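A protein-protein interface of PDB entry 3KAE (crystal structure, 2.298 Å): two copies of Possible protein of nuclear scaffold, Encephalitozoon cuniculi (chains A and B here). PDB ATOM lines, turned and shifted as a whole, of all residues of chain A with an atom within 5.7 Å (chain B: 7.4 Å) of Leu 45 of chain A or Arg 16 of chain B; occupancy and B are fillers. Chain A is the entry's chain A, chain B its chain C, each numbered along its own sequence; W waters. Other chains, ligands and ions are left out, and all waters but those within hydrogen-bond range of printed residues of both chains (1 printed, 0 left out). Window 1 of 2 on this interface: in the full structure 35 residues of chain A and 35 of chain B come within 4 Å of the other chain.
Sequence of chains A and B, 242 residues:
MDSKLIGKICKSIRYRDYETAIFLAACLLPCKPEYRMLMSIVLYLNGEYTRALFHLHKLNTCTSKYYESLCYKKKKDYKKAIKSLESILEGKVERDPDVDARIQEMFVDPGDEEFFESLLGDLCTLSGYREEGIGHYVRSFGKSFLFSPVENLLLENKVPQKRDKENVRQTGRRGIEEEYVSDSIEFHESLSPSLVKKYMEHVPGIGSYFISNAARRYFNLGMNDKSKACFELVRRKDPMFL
The backbone carbonyl oxygen (O) of Ile 13 of chain A sits close to the guanidinium group (NH1) of Arg 16 of chain A, 3.4 Å away.
The side-chain hydroxyl (OH) of Tyr 18 of chain A sits at hydrogen-bond distance from the guanidinium group (NH1) of Arg 16 of chain A, at 2.9 Å.
O of Ile 13 of chain B lies close to NH1 of Arg 16 of chain B, at 3.4 Å.
The guanidinium group (NH1) of Arg 16 of chain B sits at hydrogen-bond distance from the side-chain hydroxyl (OH) of Tyr 18 of chain B.
Arg 16 of chain A touches Leu 45 of chain B, and with the chains exchanged Leu 45 of chain A touches Arg 16 of chain B.
Tyr 18 of chain A touches Leu 45 of chain B, and with the chains exchanged Leu 45 of chain A touches Tyr 18 of chain B.
5 positions are printed for both chains.
Water W1 lies within hydrogen-bond range of the side-chain hydroxyl of Tyr 67 of chain A, the backbone carbonyl oxygen of Met 106 of chain A, the backbone carbonyl oxygen of Arg 14 of chain B and the guanidinium group of Arg 16 of chain B.
Of the 16 printed residues of chain A, 7 touch a printed residue of chain B.
Hydrophobic or aromatic side chains of chain A within 4 Å of the printed part of chain B: Tyr 18, Leu 45, Tyr 66, Tyr 67, Leu 70 and Met 106.
Of the 15 printed residues of chain B, 5 touch a printed residue of chain A.
Printed residues of chain B that touch a printed residue of chain A: Arg 14, Tyr 15, Arg 16, Tyr 18 and Leu 45.
Among the printed residues, no Asp or Glu carboxylate lies within 4 Å of a Lys or Arg side-chain nitrogen of the other chain.
Arg 16 of chain A touches Leu 45 of chain B (NH1 to CD2, 3.5 Å).
OH of Tyr 18 of chain A touches CD2 of Leu 45 of chain B (3.998 Å).
CD2 of Leu 45 of chain A touches NH1 of Arg 16 of chain B, at 3.6 Å.
Tyr 18 of chain B touches Leu 45 of chain A (OH to CD2, 3.9 Å).
Arg 14 of chain B touches Tyr 67 of chain A.
Leu 70 of chain A touches Arg 16 of chain B (CD1 to CG, 3.8 Å).
CE of Met 106 of chain A touches NH2 of Arg 16 of chain B, at 3.98 Å.
The side-chain hydroxyl (OH) of Tyr 66 of chain A is in hydrogen-bond range of the backbone carbonyl oxygen (O) of Tyr 15 of chain B.
The side-chain hydroxyl (OH) of Tyr 67 of chain A lies within hydrogen-bond range of the guanidinium group (NE) of Arg 16 of chain B, at 2.9 Å.
Printed residues of chain B within 4 Å of Tyr 18 of chain A: Leu 45.
Printed residues of chain A within 4 Å of Tyr 15 of chain B: Tyr 66 (2.7 Å).
The nearest residue of chain B that does not touch Leu 45 of chain A is Leu 45 of chain B (5.3 Å).
The nearest printed residue of chain A that does not touch Arg 16 of chain B is Tyr 44 of chain A (4.03 Å).
The nearest printed residue of chain B that does not touch Tyr 18 of chain A is Tyr 18 of chain B (6.3 Å).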
ATOM      1  N   ILE A  13      27.993 -14.930  -1.904  1.00  0.00           N
ATOM      2  CA  ILE A  13      26.771 -15.246  -2.625  1.00  0.00           C
ATOM      3  C   ILE A  13      26.401 -16.696  -2.335  1.00  0.00           C
ATOM      4  O   ILE A  13      25.312 -16.992  -1.849  1.00  0.00           O
ATOM      5  CB  ILE A  13      26.937 -15.026  -4.118  1.00  0.00           C
ATOM      6  CG1 ILE A  13      27.072 -13.531  -4.407  1.00  0.00           C
ATOM      7  CG2 ILE A  13      25.723 -15.596  -4.860  1.00  0.00           C
ATOM      8  CD1 ILE A  13      27.871 -13.220  -5.667  1.00  0.00           C
ATOM      9  N   ARG A  16      24.842 -16.925   0.731  1.00  0.00           N
ATOM     10  CA  ARG A  16      23.636 -16.103   0.891  1.00  0.00           C
ATOM     11  C   ARG A  16      23.871 -14.958   1.894  1.00  0.00           C
ATOM     12  O   ARG A  16      22.919 -14.398   2.478  1.00  0.00           O
ATOM     13  CB  ARG A  16      22.417 -16.954   1.310  1.00  0.00           C
ATOM     14  CG  ARG A  16      22.203 -18.239   0.452  1.00  0.00           C
ATOM     15  CD  ARG A  16      21.938 -17.956  -1.031  1.00  0.00           C
ATOM     16  NE  ARG A  16      22.469 -19.025  -1.868  1.00  0.00           N
ATOM     17  CZ  ARG A  16      22.771 -18.911  -3.156  1.00  0.00           C
ATOM     18  NH1 ARG A  16      22.612 -17.757  -3.788  1.00  0.00           N
ATOM     19  NH2 ARG A  16      23.269 -19.953  -3.805  1.00  0.00           N
ATOM     20  N   TYR A  18      24.448 -11.693   1.594  1.00  0.00           N
ATOM     21  CA  TYR A  18      24.361 -10.718   0.518  1.00  0.00           C
ATOM     22  C   TYR A  18      24.873  -9.323   0.947  1.00  0.00           C
ATOM     23  O   TYR A  18      25.513  -8.625   0.151  1.00  0.00           O
ATOM     24  CB  TYR A  18      22.925 -10.653  -0.039  1.00  0.00           C
ATOM     25  CG  TYR A  18      22.448 -11.930  -0.764  1.00  0.00           C
ATOM     26  CD1 TYR A  18      23.297 -12.626  -1.606  1.00  0.00           C
ATOM     27  CD2 TYR A  18      21.152 -12.408  -0.616  1.00  0.00           C
ATOM     28  CE1 TYR A  18      22.896 -13.743  -2.279  1.00  0.00           C
ATOM     29  CE2 TYR A  18      20.735 -13.561  -1.272  1.00  0.00           C
ATOM     30  CZ  TYR A  18      21.620 -14.217  -2.112  1.00  0.00           C
ATOM     31  OH  TYR A  18      21.260 -15.336  -2.815  1.00  0.00           O
ATOM     32  N   SER A  40      24.667  -4.975  -9.307  1.00  0.00           N
ATOM     33  CA  SER A  40      23.252  -5.033  -9.653  1.00  0.00           C
ATOM     34  C   SER A  40      22.648  -6.401  -9.315  1.00  0.00           C
ATOM     35  O   SER A  40      21.560  -6.488  -8.755  1.00  0.00           O
ATOM     36  CB  SER A  40      23.068  -4.753 -11.143  1.00  0.00           C
ATOM     37  OG  SER A  40      23.263  -3.394 -11.437  1.00  0.00           O
ATOM     38  N   ILE A  41      23.368  -7.460  -9.668  1.00  0.00           N
ATOM     39  CA  ILE A  41      22.935  -8.825  -9.405  1.00  0.00           C
ATOM     40  C   ILE A  41      22.747  -9.114  -7.918  1.00  0.00           C
ATOM     41  O   ILE A  41      21.652  -9.480  -7.469  1.00  0.00           O
ATOM     42  CB  ILE A  41      23.904  -9.841 -10.046  1.00  0.00           C
ATOM     43  CG1 ILE A  41      23.859  -9.684 -11.575  1.00  0.00           C
ATOM     44  CG2 ILE A  41      23.526 -11.276  -9.657  1.00  0.00           C
ATOM     45  CD1 ILE A  41      24.644 -10.719 -12.336  1.00  0.00           C
ATOM     46  N   VAL A  42      23.815  -8.919  -7.155  1.00  0.00           N
ATOM     47  CA  VAL A  42      23.768  -9.112  -5.714  1.00  0.00           C
ATOM     48  C   VAL A  42      22.662  -8.277  -5.044  1.00  0.00           C
ATOM     49  O   VAL A  42      22.005  -8.723  -4.105  1.00  0.00           O
ATOM     50  CB  VAL A  42      25.148  -8.871  -5.075  1.00  0.00           C
ATOM     51  CG1 VAL A  42      25.056  -8.991  -3.589  1.00  0.00           C
ATOM     52  CG2 VAL A  42      26.171  -9.874  -5.630  1.00  0.00           C
ATOM     53  N   LEU A  43      22.404  -7.095  -5.574  1.00  0.00           N
ATOM     54  CA  LEU A  43      21.313  -6.268  -5.081  1.00  0.00           C
ATOM     55  C   LEU A  43      19.968  -6.931  -5.439  1.00  0.00           C
ATOM     56  O   LEU A  43      19.013  -6.944  -4.649  1.00  0.00           O
ATOM     57  CB  LEU A  43      21.420  -4.875  -5.719  1.00  0.00           C
ATOM     58  CG  LEU A  43      21.456  -3.573  -4.903  1.00  0.00           C
ATOM     59  CD1 LEU A  43      21.995  -3.749  -3.509  1.00  0.00           C
ATOM     60  CD2 LEU A  43      22.293  -2.520  -5.647  1.00  0.00           C
ATOM     61  N   TYR A  44      19.889  -7.479  -6.650  1.00  0.00           N
ATOM     62  CA  TYR A  44      18.688  -8.189  -7.060  1.00  0.00           C
ATOM     63  C   TYR A  44      18.448  -9.391  -6.139  1.00  0.00           C
ATOM     64  O   TYR A  44      17.353  -9.579  -5.615  1.00  0.00           O
ATOM     65  CB  TYR A  44      18.761  -8.648  -8.521  1.00  0.00           C
ATOM     66  CG  TYR A  44      17.554  -9.480  -8.912  1.00  0.00           C
ATOM     67  CD1 TYR A  44      16.392  -8.878  -9.391  1.00  0.00           C
ATOM     68  CD2 TYR A  44      17.554 -10.852  -8.745  1.00  0.00           C
ATOM     69  CE1 TYR A  44      15.276  -9.629  -9.724  1.00  0.00           C
ATOM     70  CE2 TYR A  44      16.434 -11.619  -9.080  1.00  0.00           C
ATOM     71  CZ  TYR A  44      15.306 -11.000  -9.567  1.00  0.00           C
ATOM     72  OH  TYR A  44      14.204 -11.753  -9.891  1.00  0.00           O
ATOM     73  N   LEU A  45      19.489 -10.186  -5.918  1.00  0.00           N
ATOM     74  CA  LEU A  45      19.364 -11.369  -5.065  1.00  0.00           C
ATOM     75  C   LEU A  45      18.925 -11.007  -3.654  1.00  0.00           C
ATOM     76  O   LEU A  45      18.242 -11.788  -3.001  1.00  0.00           O
ATOM     77  CB  LEU A  45      20.673 -12.152  -5.022  1.00  0.00           C
ATOM     78  CG  LEU A  45      21.062 -12.818  -6.340  1.00  0.00           C
ATOM     79  CD1 LEU A  45      22.476 -13.390  -6.273  1.00  0.00           C
ATOM     80  CD2 LEU A  45      20.050 -13.909  -6.677  1.00  0.00           C
ATOM     81  N   ASN A  46      19.299  -9.816  -3.196  1.00  0.00           N
ATOM     82  CA  ASN A  46      18.986  -9.398  -1.829  1.00  0.00           C
ATOM     83  C   ASN A  46      17.597  -8.776  -1.742  1.00  0.00           C
ATOM     84  O   ASN A  46      17.196  -8.248  -0.707  1.00  0.00           O
ATOM     85  CB  ASN A  46      20.047  -8.423  -1.300  1.00  0.00           C
ATOM     86  CG  ASN A  46      19.948  -8.219   0.203  1.00  0.00           C
ATOM     87  OD1 ASN A  46      20.095  -7.092   0.721  1.00  0.00           O
ATOM     88  ND2 ASN A  46      19.679  -9.307   0.913  1.00  0.00           N
ATOM     89  N   GLY A  47      16.866  -8.822  -2.847  1.00  0.00           N
ATOM     90  CA  GLY A  47      15.507  -8.302  -2.870  1.00  0.00           C
ATOM     91  C   GLY A  47      15.411  -6.801  -3.105  1.00  0.00           C
ATOM     92  O   GLY A  47      14.338  -6.228  -2.913  1.00  0.00           O
ATOM     93  N   GLU A  48      16.508  -6.161  -3.530  1.00  0.00           N
ATOM     94  CA  GLU A  48      16.543  -4.690  -3.622  1.00  0.00           C
ATOM     95  C   GLU A  48      16.488  -4.187  -5.056  1.00  0.00           C
ATOM     96  O   GLU A  48      17.508  -3.783  -5.633  1.00  0.00           O
ATOM     97  CB  GLU A  48      17.768  -4.116  -2.908  1.00  0.00           C
ATOM     98  CG  GLU A  48      17.835  -4.481  -1.447  1.00  0.00           C
ATOM     99  CD  GLU A  48      18.993  -3.817  -0.727  1.00  0.00           C
ATOM    100  OE1 GLU A  48      19.972  -4.523  -0.404  1.00  0.00           O
ATOM    101  OE2 GLU A  48      18.918  -2.593  -0.492  1.00  0.00           O
ATOM    102  N   TYR A  66      18.318  -7.578 -19.103  1.00  0.00           N
ATOM    103  CA  TYR A  66      17.614  -8.704 -18.520  1.00  0.00           C
ATOM    104  C   TYR A  66      17.266  -8.479 -17.038  1.00  0.00           C
ATOM    105  O   TYR A  66      16.098  -8.577 -16.646  1.00  0.00           O
ATOM    106  CB  TYR A  66      18.397  -9.996 -18.725  1.00  0.00           C
ATOM    107  CG  TYR A  66      17.604 -11.212 -18.304  1.00  0.00           C
ATOM    108  CD1 TYR A  66      16.489 -11.645 -19.041  1.00  0.00           C
ATOM    109  CD2 TYR A  66      17.959 -11.918 -17.168  1.00  0.00           C
ATOM    110  CE1 TYR A  66      15.755 -12.756 -18.634  1.00  0.00           C
ATOM    111  CE2 TYR A  66      17.246 -13.008 -16.761  1.00  0.00           C
ATOM    112  CZ  TYR A  66      16.153 -13.429 -17.492  1.00  0.00           C
ATOM    113  OH  TYR A  66      15.487 -14.513 -17.033  1.00  0.00           O
ATOM    114  N   TYR A  67      18.269  -8.165 -16.216  1.00  0.00           N
ATOM    115  CA  TYR A  67      18.016  -7.898 -14.796  1.00  0.00           C
ATOM    116  C   TYR A  67      17.142  -6.669 -14.623  1.00  0.00           C
ATOM    117  O   TYR A  67      16.361  -6.561 -13.681  1.00  0.00           O
ATOM    118  CB  TYR A  67      19.330  -7.761 -14.012  1.00  0.00           C
ATOM    119  CG  TYR A  67      19.813  -9.111 -13.554  1.00  0.00           C
ATOM    120  CD1 TYR A  67      20.642  -9.875 -14.354  1.00  0.00           C
ATOM    121  CD2 TYR A  67      19.391  -9.649 -12.339  1.00  0.00           C
ATOM    122  CE1 TYR A  67      21.071 -11.133 -13.946  1.00  0.00           C
ATOM    123  CE2 TYR A  67      19.805 -10.919 -11.925  1.00  0.00           C
ATOM    124  CZ  TYR A  67      20.645 -11.650 -12.731  1.00  0.00           C
ATOM    125  OH  TYR A  67      21.083 -12.891 -12.324  1.00  0.00           O
ATOM    126  N   LEU A  70      13.731  -7.954 -14.928  1.00  0.00           N
ATOM    127  CA  LEU A  70      13.342  -8.664 -13.719  1.00  0.00           C
ATOM    128  C   LEU A  70      12.928  -7.708 -12.623  1.00  0.00           C
ATOM    129  O   LEU A  70      11.908  -7.937 -11.953  1.00  0.00           O
ATOM    130  CB  LEU A  70      14.447  -9.584 -13.215  1.00  0.00           C
ATOM    131  CG  LEU A  70      14.967 -10.697 -14.129  1.00  0.00           C
ATOM    132  CD1 LEU A  70      16.076 -11.490 -13.417  1.00  0.00           C
ATOM    133  CD2 LEU A  70      13.836 -11.606 -14.517  1.00  0.00           C
ATOM    134  N   MET A 106      27.662 -15.705 -14.405  1.00  0.00           N
ATOM    135  CA  MET A 106      26.409 -15.125 -13.938  1.00  0.00           C
ATOM    136  C   MET A 106      25.771 -14.291 -15.028  1.00  0.00           C
ATOM    137  O   MET A 106      24.726 -13.675 -14.819  1.00  0.00           O
ATOM    138  CB  MET A 106      26.637 -14.241 -12.714  1.00  0.00           C
ATOM    139  CG  MET A 106      27.592 -14.810 -11.688  1.00  0.00           C
ATOM    140  SD  MET A 106      27.476 -13.885 -10.144  1.00  0.00           S
ATOM    141  CE  MET A 106      25.853 -14.408  -9.595  1.00  0.00           C
ATOM    142  N   CYS B  10      20.989 -25.429 -13.878  1.00  0.00           N
ATOM    143  CA  CYS B  10      21.965 -24.368 -13.666  1.00  0.00           C
ATOM    144  C   CYS B  10      21.598 -23.174 -14.518  1.00  0.00           C
ATOM    145  O   CYS B  10      21.578 -22.031 -14.046  1.00  0.00           O
ATOM    146  CB  CYS B  10      23.363 -24.844 -14.024  1.00  0.00           C
ATOM    147  SG  CYS B  10      23.992 -26.060 -12.858  1.00  0.00           S
ATOM    148  N   LYS B  11      21.271 -23.447 -15.775  1.00  0.00           N
ATOM    149  CA  LYS B  11      20.888 -22.375 -16.671  1.00  0.00           C
ATOM    150  C   LYS B  11      19.653 -21.628 -16.194  1.00  0.00           C
ATOM    151  O   LYS B  11      19.575 -20.403 -16.327  1.00  0.00           O
ATOM    152  CB  LYS B  11      20.707 -22.877 -18.106  1.00  0.00           C
ATOM    153  CG  LYS B  11      20.696 -21.738 -19.109  1.00  0.00           C
ATOM    154  CD  LYS B  11      20.563 -22.234 -20.535  1.00  0.00           C
ATOM    155  CE  LYS B  11      21.838 -22.896 -21.029  1.00  0.00           C
ATOM    156  NZ  LYS B  11      21.696 -23.360 -22.443  1.00  0.00           N
ATOM    157  N   SER B  12      18.698 -22.354 -15.619  1.00  0.00           N
ATOM    158  CA  SER B  12      17.485 -21.726 -15.104  1.00  0.00           C
ATOM    159  C   SER B  12      17.745 -20.874 -13.861  1.00  0.00           C
ATOM    160  O   SER B  12      17.055 -19.869 -13.627  1.00  0.00           O
ATOM    161  CB  SER B  12      16.424 -22.792 -14.773  1.00  0.00           C
ATOM    162  OG  SER B  12      16.183 -23.637 -15.876  1.00  0.00           O
ATOM    163  N   ILE B  13      18.705 -21.307 -13.045  1.00  0.00           N
ATOM    164  CA  ILE B  13      19.068 -20.545 -11.853  1.00  0.00           C
ATOM    165  C   ILE B  13      19.712 -19.227 -12.291  1.00  0.00           C
ATOM    166  O   ILE B  13      19.265 -18.158 -11.915  1.00  0.00           O
ATOM    167  CB  ILE B  13      20.007 -21.353 -10.954  1.00  0.00           C
ATOM    168  CG1 ILE B  13      19.225 -22.531 -10.355  1.00  0.00           C
ATOM    169  CG2 ILE B  13      20.600 -20.456  -9.866  1.00  0.00           C
ATOM    170  CD1 ILE B  13      20.060 -23.756 -10.036  1.00  0.00           C
ATOM    171  N   ARG B  14      20.728 -19.341 -13.140  1.00  0.00           N
ATOM    172  CA  ARG B  14      21.379 -18.195 -13.757  1.00  0.00           C
ATOM    173  C   ARG B  14      20.390 -17.225 -14.389  1.00  0.00           C
ATOM    174  O   ARG B  14      20.641 -16.035 -14.421  1.00  0.00           O
ATOM    175  CB  ARG B  14      22.438 -18.654 -14.759  1.00  0.00           C
ATOM    176  CG  ARG B  14      22.730 -17.664 -15.858  1.00  0.00           C
ATOM    177  CD  ARG B  14      24.081 -17.940 -16.498  1.00  0.00           C
ATOM    178  NE  ARG B  14      24.068 -19.080 -17.405  1.00  0.00           N
ATOM    179  CZ  ARG B  14      24.131 -18.979 -18.731  1.00  0.00           C
ATOM    180  NH1 ARG B  14      24.216 -17.789 -19.308  1.00  0.00           N
ATOM    181  NH2 ARG B  14      24.116 -20.074 -19.485  1.00  0.00           N
ATOM    182  N   TYR B  15      19.242 -17.709 -14.853  1.00  0.00           N
ATOM    183  CA  TYR B  15      18.238 -16.802 -15.430  1.00  0.00           C
ATOM    184  C   TYR B  15      17.155 -16.426 -14.428  1.00  0.00           C
ATOM    185  O   TYR B  15      16.221 -15.684 -14.739  1.00  0.00           O
ATOM    186  CB  TYR B  15      17.633 -17.383 -16.722  1.00  0.00           C
ATOM    187  CG  TYR B  15      18.542 -17.218 -17.931  1.00  0.00           C
ATOM    188  CD1 TYR B  15      19.518 -18.157 -18.220  1.00  0.00           C
ATOM    189  CD2 TYR B  15      18.430 -16.105 -18.769  1.00  0.00           C
ATOM    190  CE1 TYR B  15      20.355 -18.010 -19.317  1.00  0.00           C
ATOM    191  CE2 TYR B  15      19.270 -15.939 -19.864  1.00  0.00           C
ATOM    192  CZ  TYR B  15      20.230 -16.897 -20.129  1.00  0.00           C
ATOM    193  OH  TYR B  15      21.064 -16.747 -21.210  1.00  0.00           O
ATOM    194  N   ARG B  16      17.284 -16.931 -13.211  1.00  0.00           N
ATOM    195  CA  ARG B  16      16.348 -16.599 -12.148  1.00  0.00           C
ATOM    196  C   ARG B  16      14.982 -17.129 -12.522  1.00  0.00           C
ATOM    197  O   ARG B  16      13.948 -16.661 -12.032  1.00  0.00           O
ATOM    198  CB  ARG B  16      16.316 -15.082 -11.848  1.00  0.00           C
ATOM    199  CG  ARG B  16      17.705 -14.451 -11.643  1.00  0.00           C
ATOM    200  CD  ARG B  16      18.471 -15.059 -10.449  1.00  0.00           C
ATOM    201  NE  ARG B  16      19.905 -14.964 -10.662  1.00  0.00           N
ATOM    202  CZ  ARG B  16      20.807 -15.686 -10.009  1.00  0.00           C
ATOM    203  NH1 ARG B  16      20.412 -16.550  -9.091  1.00  0.00           N
ATOM    204  NH2 ARG B  16      22.100 -15.545 -10.281  1.00  0.00           N
ATOM    205  N   ASP B  17      14.989 -18.129 -13.396  1.00  0.00           N
ATOM    206  CA  ASP B  17      13.779 -18.872 -13.732  1.00  0.00           C
ATOM    207  C   ASP B  17      13.662 -20.077 -12.782  1.00  0.00           C
ATOM    208  O   ASP B  17      14.020 -21.215 -13.135  1.00  0.00           O
ATOM    209  CB  ASP B  17      13.816 -19.354 -15.184  1.00  0.00           C
ATOM    210  CG  ASP B  17      12.593 -20.188 -15.551  1.00  0.00           C
ATOM    211  OD1 ASP B  17      11.627 -20.251 -14.747  1.00  0.00           O
ATOM    212  OD2 ASP B  17      12.601 -20.794 -16.643  1.00  0.00           O
ATOM    213  N   TYR B  18      13.167 -19.810 -11.580  1.00  0.00           N
ATOM    214  CA  TYR B  18      13.244 -20.766 -10.485  1.00  0.00           C
ATOM    215  C   TYR B  18      12.167 -21.845 -10.606  1.00  0.00           C
ATOM    216  O   TYR B  18      12.431 -23.000 -10.302  1.00  0.00           O
ATOM    217  CB  TYR B  18      13.174 -20.043  -9.121  1.00  0.00           C
ATOM    218  CG  TYR B  18      14.396 -19.161  -8.792  1.00  0.00           C
ATOM    219  CD1 TYR B  18      15.687 -19.588  -9.106  1.00  0.00           C
ATOM    220  CD2 TYR B  18      14.253 -17.920  -8.136  1.00  0.00           C
ATOM    221  CE1 TYR B  18      16.797 -18.818  -8.806  1.00  0.00           C
ATOM    222  CE2 TYR B  18      15.379 -17.123  -7.830  1.00  0.00           C
ATOM    223  CZ  TYR B  18      16.642 -17.594  -8.163  1.00  0.00           C
ATOM    224  OH  TYR B  18      17.767 -16.861  -7.878  1.00  0.00           O
ATOM    225  N   GLU B  19      10.968 -21.470 -11.052  1.00  0.00           N
ATOM    226  CA  GLU B  19       9.895 -22.455 -11.311  1.00  0.00           C
ATOM    227  C   GLU B  19      10.377 -23.599 -12.210  1.00  0.00           C
ATOM    228  O   GLU B  19      10.190 -24.779 -11.916  1.00  0.00           O
ATOM    229  CB  GLU B  19       8.667 -21.788 -11.921  1.00  0.00           C
ATOM    230  CG  GLU B  19       8.001 -20.731 -11.015  1.00  0.00           C
ATOM    231  CD  GLU B  19       7.614 -21.281  -9.656  1.00  0.00           C
ATOM    232  OE1 GLU B  19       7.647 -22.512  -9.479  1.00  0.00           O
ATOM    233  OE2 GLU B  19       7.272 -20.483  -8.758  1.00  0.00           O
ATOM    234  N   THR B  20      11.050 -23.263 -13.291  1.00  0.00           N
ATOM    235  CA  THR B  20      11.617 -24.300 -14.138  1.00  0.00           C
ATOM    236  C   THR B  20      12.615 -25.159 -13.375  1.00  0.00           C
ATOM    237  O   THR B  20      12.613 -26.375 -13.494  1.00  0.00           O
ATOM    238  CB  THR B  20      12.292 -23.694 -15.366  1.00  0.00           C
ATOM    239  OG1 THR B  20      11.309 -22.989 -16.121  1.00  0.00           O
ATOM    240  CG2 THR B  20      12.927 -24.750 -16.213  1.00  0.00           C
ATOM    241  N   ALA B  21      13.466 -24.526 -12.582  1.00  0.00           N
ATOM    242  CA  ALA B  21      14.503 -25.245 -11.848  1.00  0.00           C
ATOM    243  C   ALA B  21      13.909 -26.166 -10.801  1.00  0.00           C
ATOM    244  O   ALA B  21      14.410 -27.257 -10.569  1.00  0.00           O
ATOM    245  CB  ALA B  21      15.476 -24.238 -11.187  1.00  0.00           C
ATOM    246  N   LEU B  45      15.992 -20.248  -2.897  1.00  0.00           N
ATOM    247  CA  LEU B  45      16.149 -19.108  -3.788  1.00  0.00           C
ATOM    248  C   LEU B  45      14.817 -18.530  -4.236  1.00  0.00           C
ATOM    249  O   LEU B  45      14.709 -17.333  -4.493  1.00  0.00           O
ATOM    250  CB  LEU B  45      17.005 -19.467  -4.997  1.00  0.00           C
ATOM    251  CG  LEU B  45      18.474 -19.758  -4.677  1.00  0.00           C
ATOM    252  CD1 LEU B  45      19.180 -20.376  -5.894  1.00  0.00           C
ATOM    253  CD2 LEU B  45      19.202 -18.480  -4.181  1.00  0.00           C
ATOM    254  N   ASN B  46      13.796 -19.379  -4.320  1.00  0.00           N
ATOM    255  CA  ASN B  46      12.499 -18.932  -4.804  1.00  0.00           C
ATOM    256  C   ASN B  46      11.645 -18.385  -3.677  1.00  0.00           C
ATOM    257  O   ASN B  46      10.464 -18.085  -3.862  1.00  0.00           O
ATOM    258  CB  ASN B  46      11.775 -20.059  -5.545  1.00  0.00           C
ATOM    259  CG  ASN B  46      10.592 -19.558  -6.344  1.00  0.00           C
ATOM    260  OD1 ASN B  46       9.517 -20.177  -6.361  1.00  0.00           O
ATOM    261  ND2 ASN B  46      10.775 -18.421  -7.006  1.00  0.00           N
ATOM    262  N   LYS B  74      14.582 -17.168   8.275  1.00  0.00           N
ATOM    263  CA  LYS B  74      13.523 -16.481   7.533  1.00  0.00           C
ATOM    264  C   LYS B  74      12.179 -16.608   8.244  1.00  0.00           C
ATOM    265  O   LYS B  74      11.351 -15.700   8.210  1.00  0.00           O
ATOM    266  CB  LYS B  74      13.390 -17.062   6.130  1.00  0.00           C
ATOM    267  CG  LYS B  74      14.516 -16.734   5.202  1.00  0.00           C
ATOM    268  CD  LYS B  74      14.595 -15.250   4.952  1.00  0.00           C
ATOM    269  CE  LYS B  74      15.739 -14.942   4.016  1.00  0.00           C
ATOM    270  NZ  LYS B  74      15.786 -13.496   3.654  1.00  0.00           N
HETATM  271  O   HOH W   1      22.683 -14.504 -13.251  1.00  0.00           O
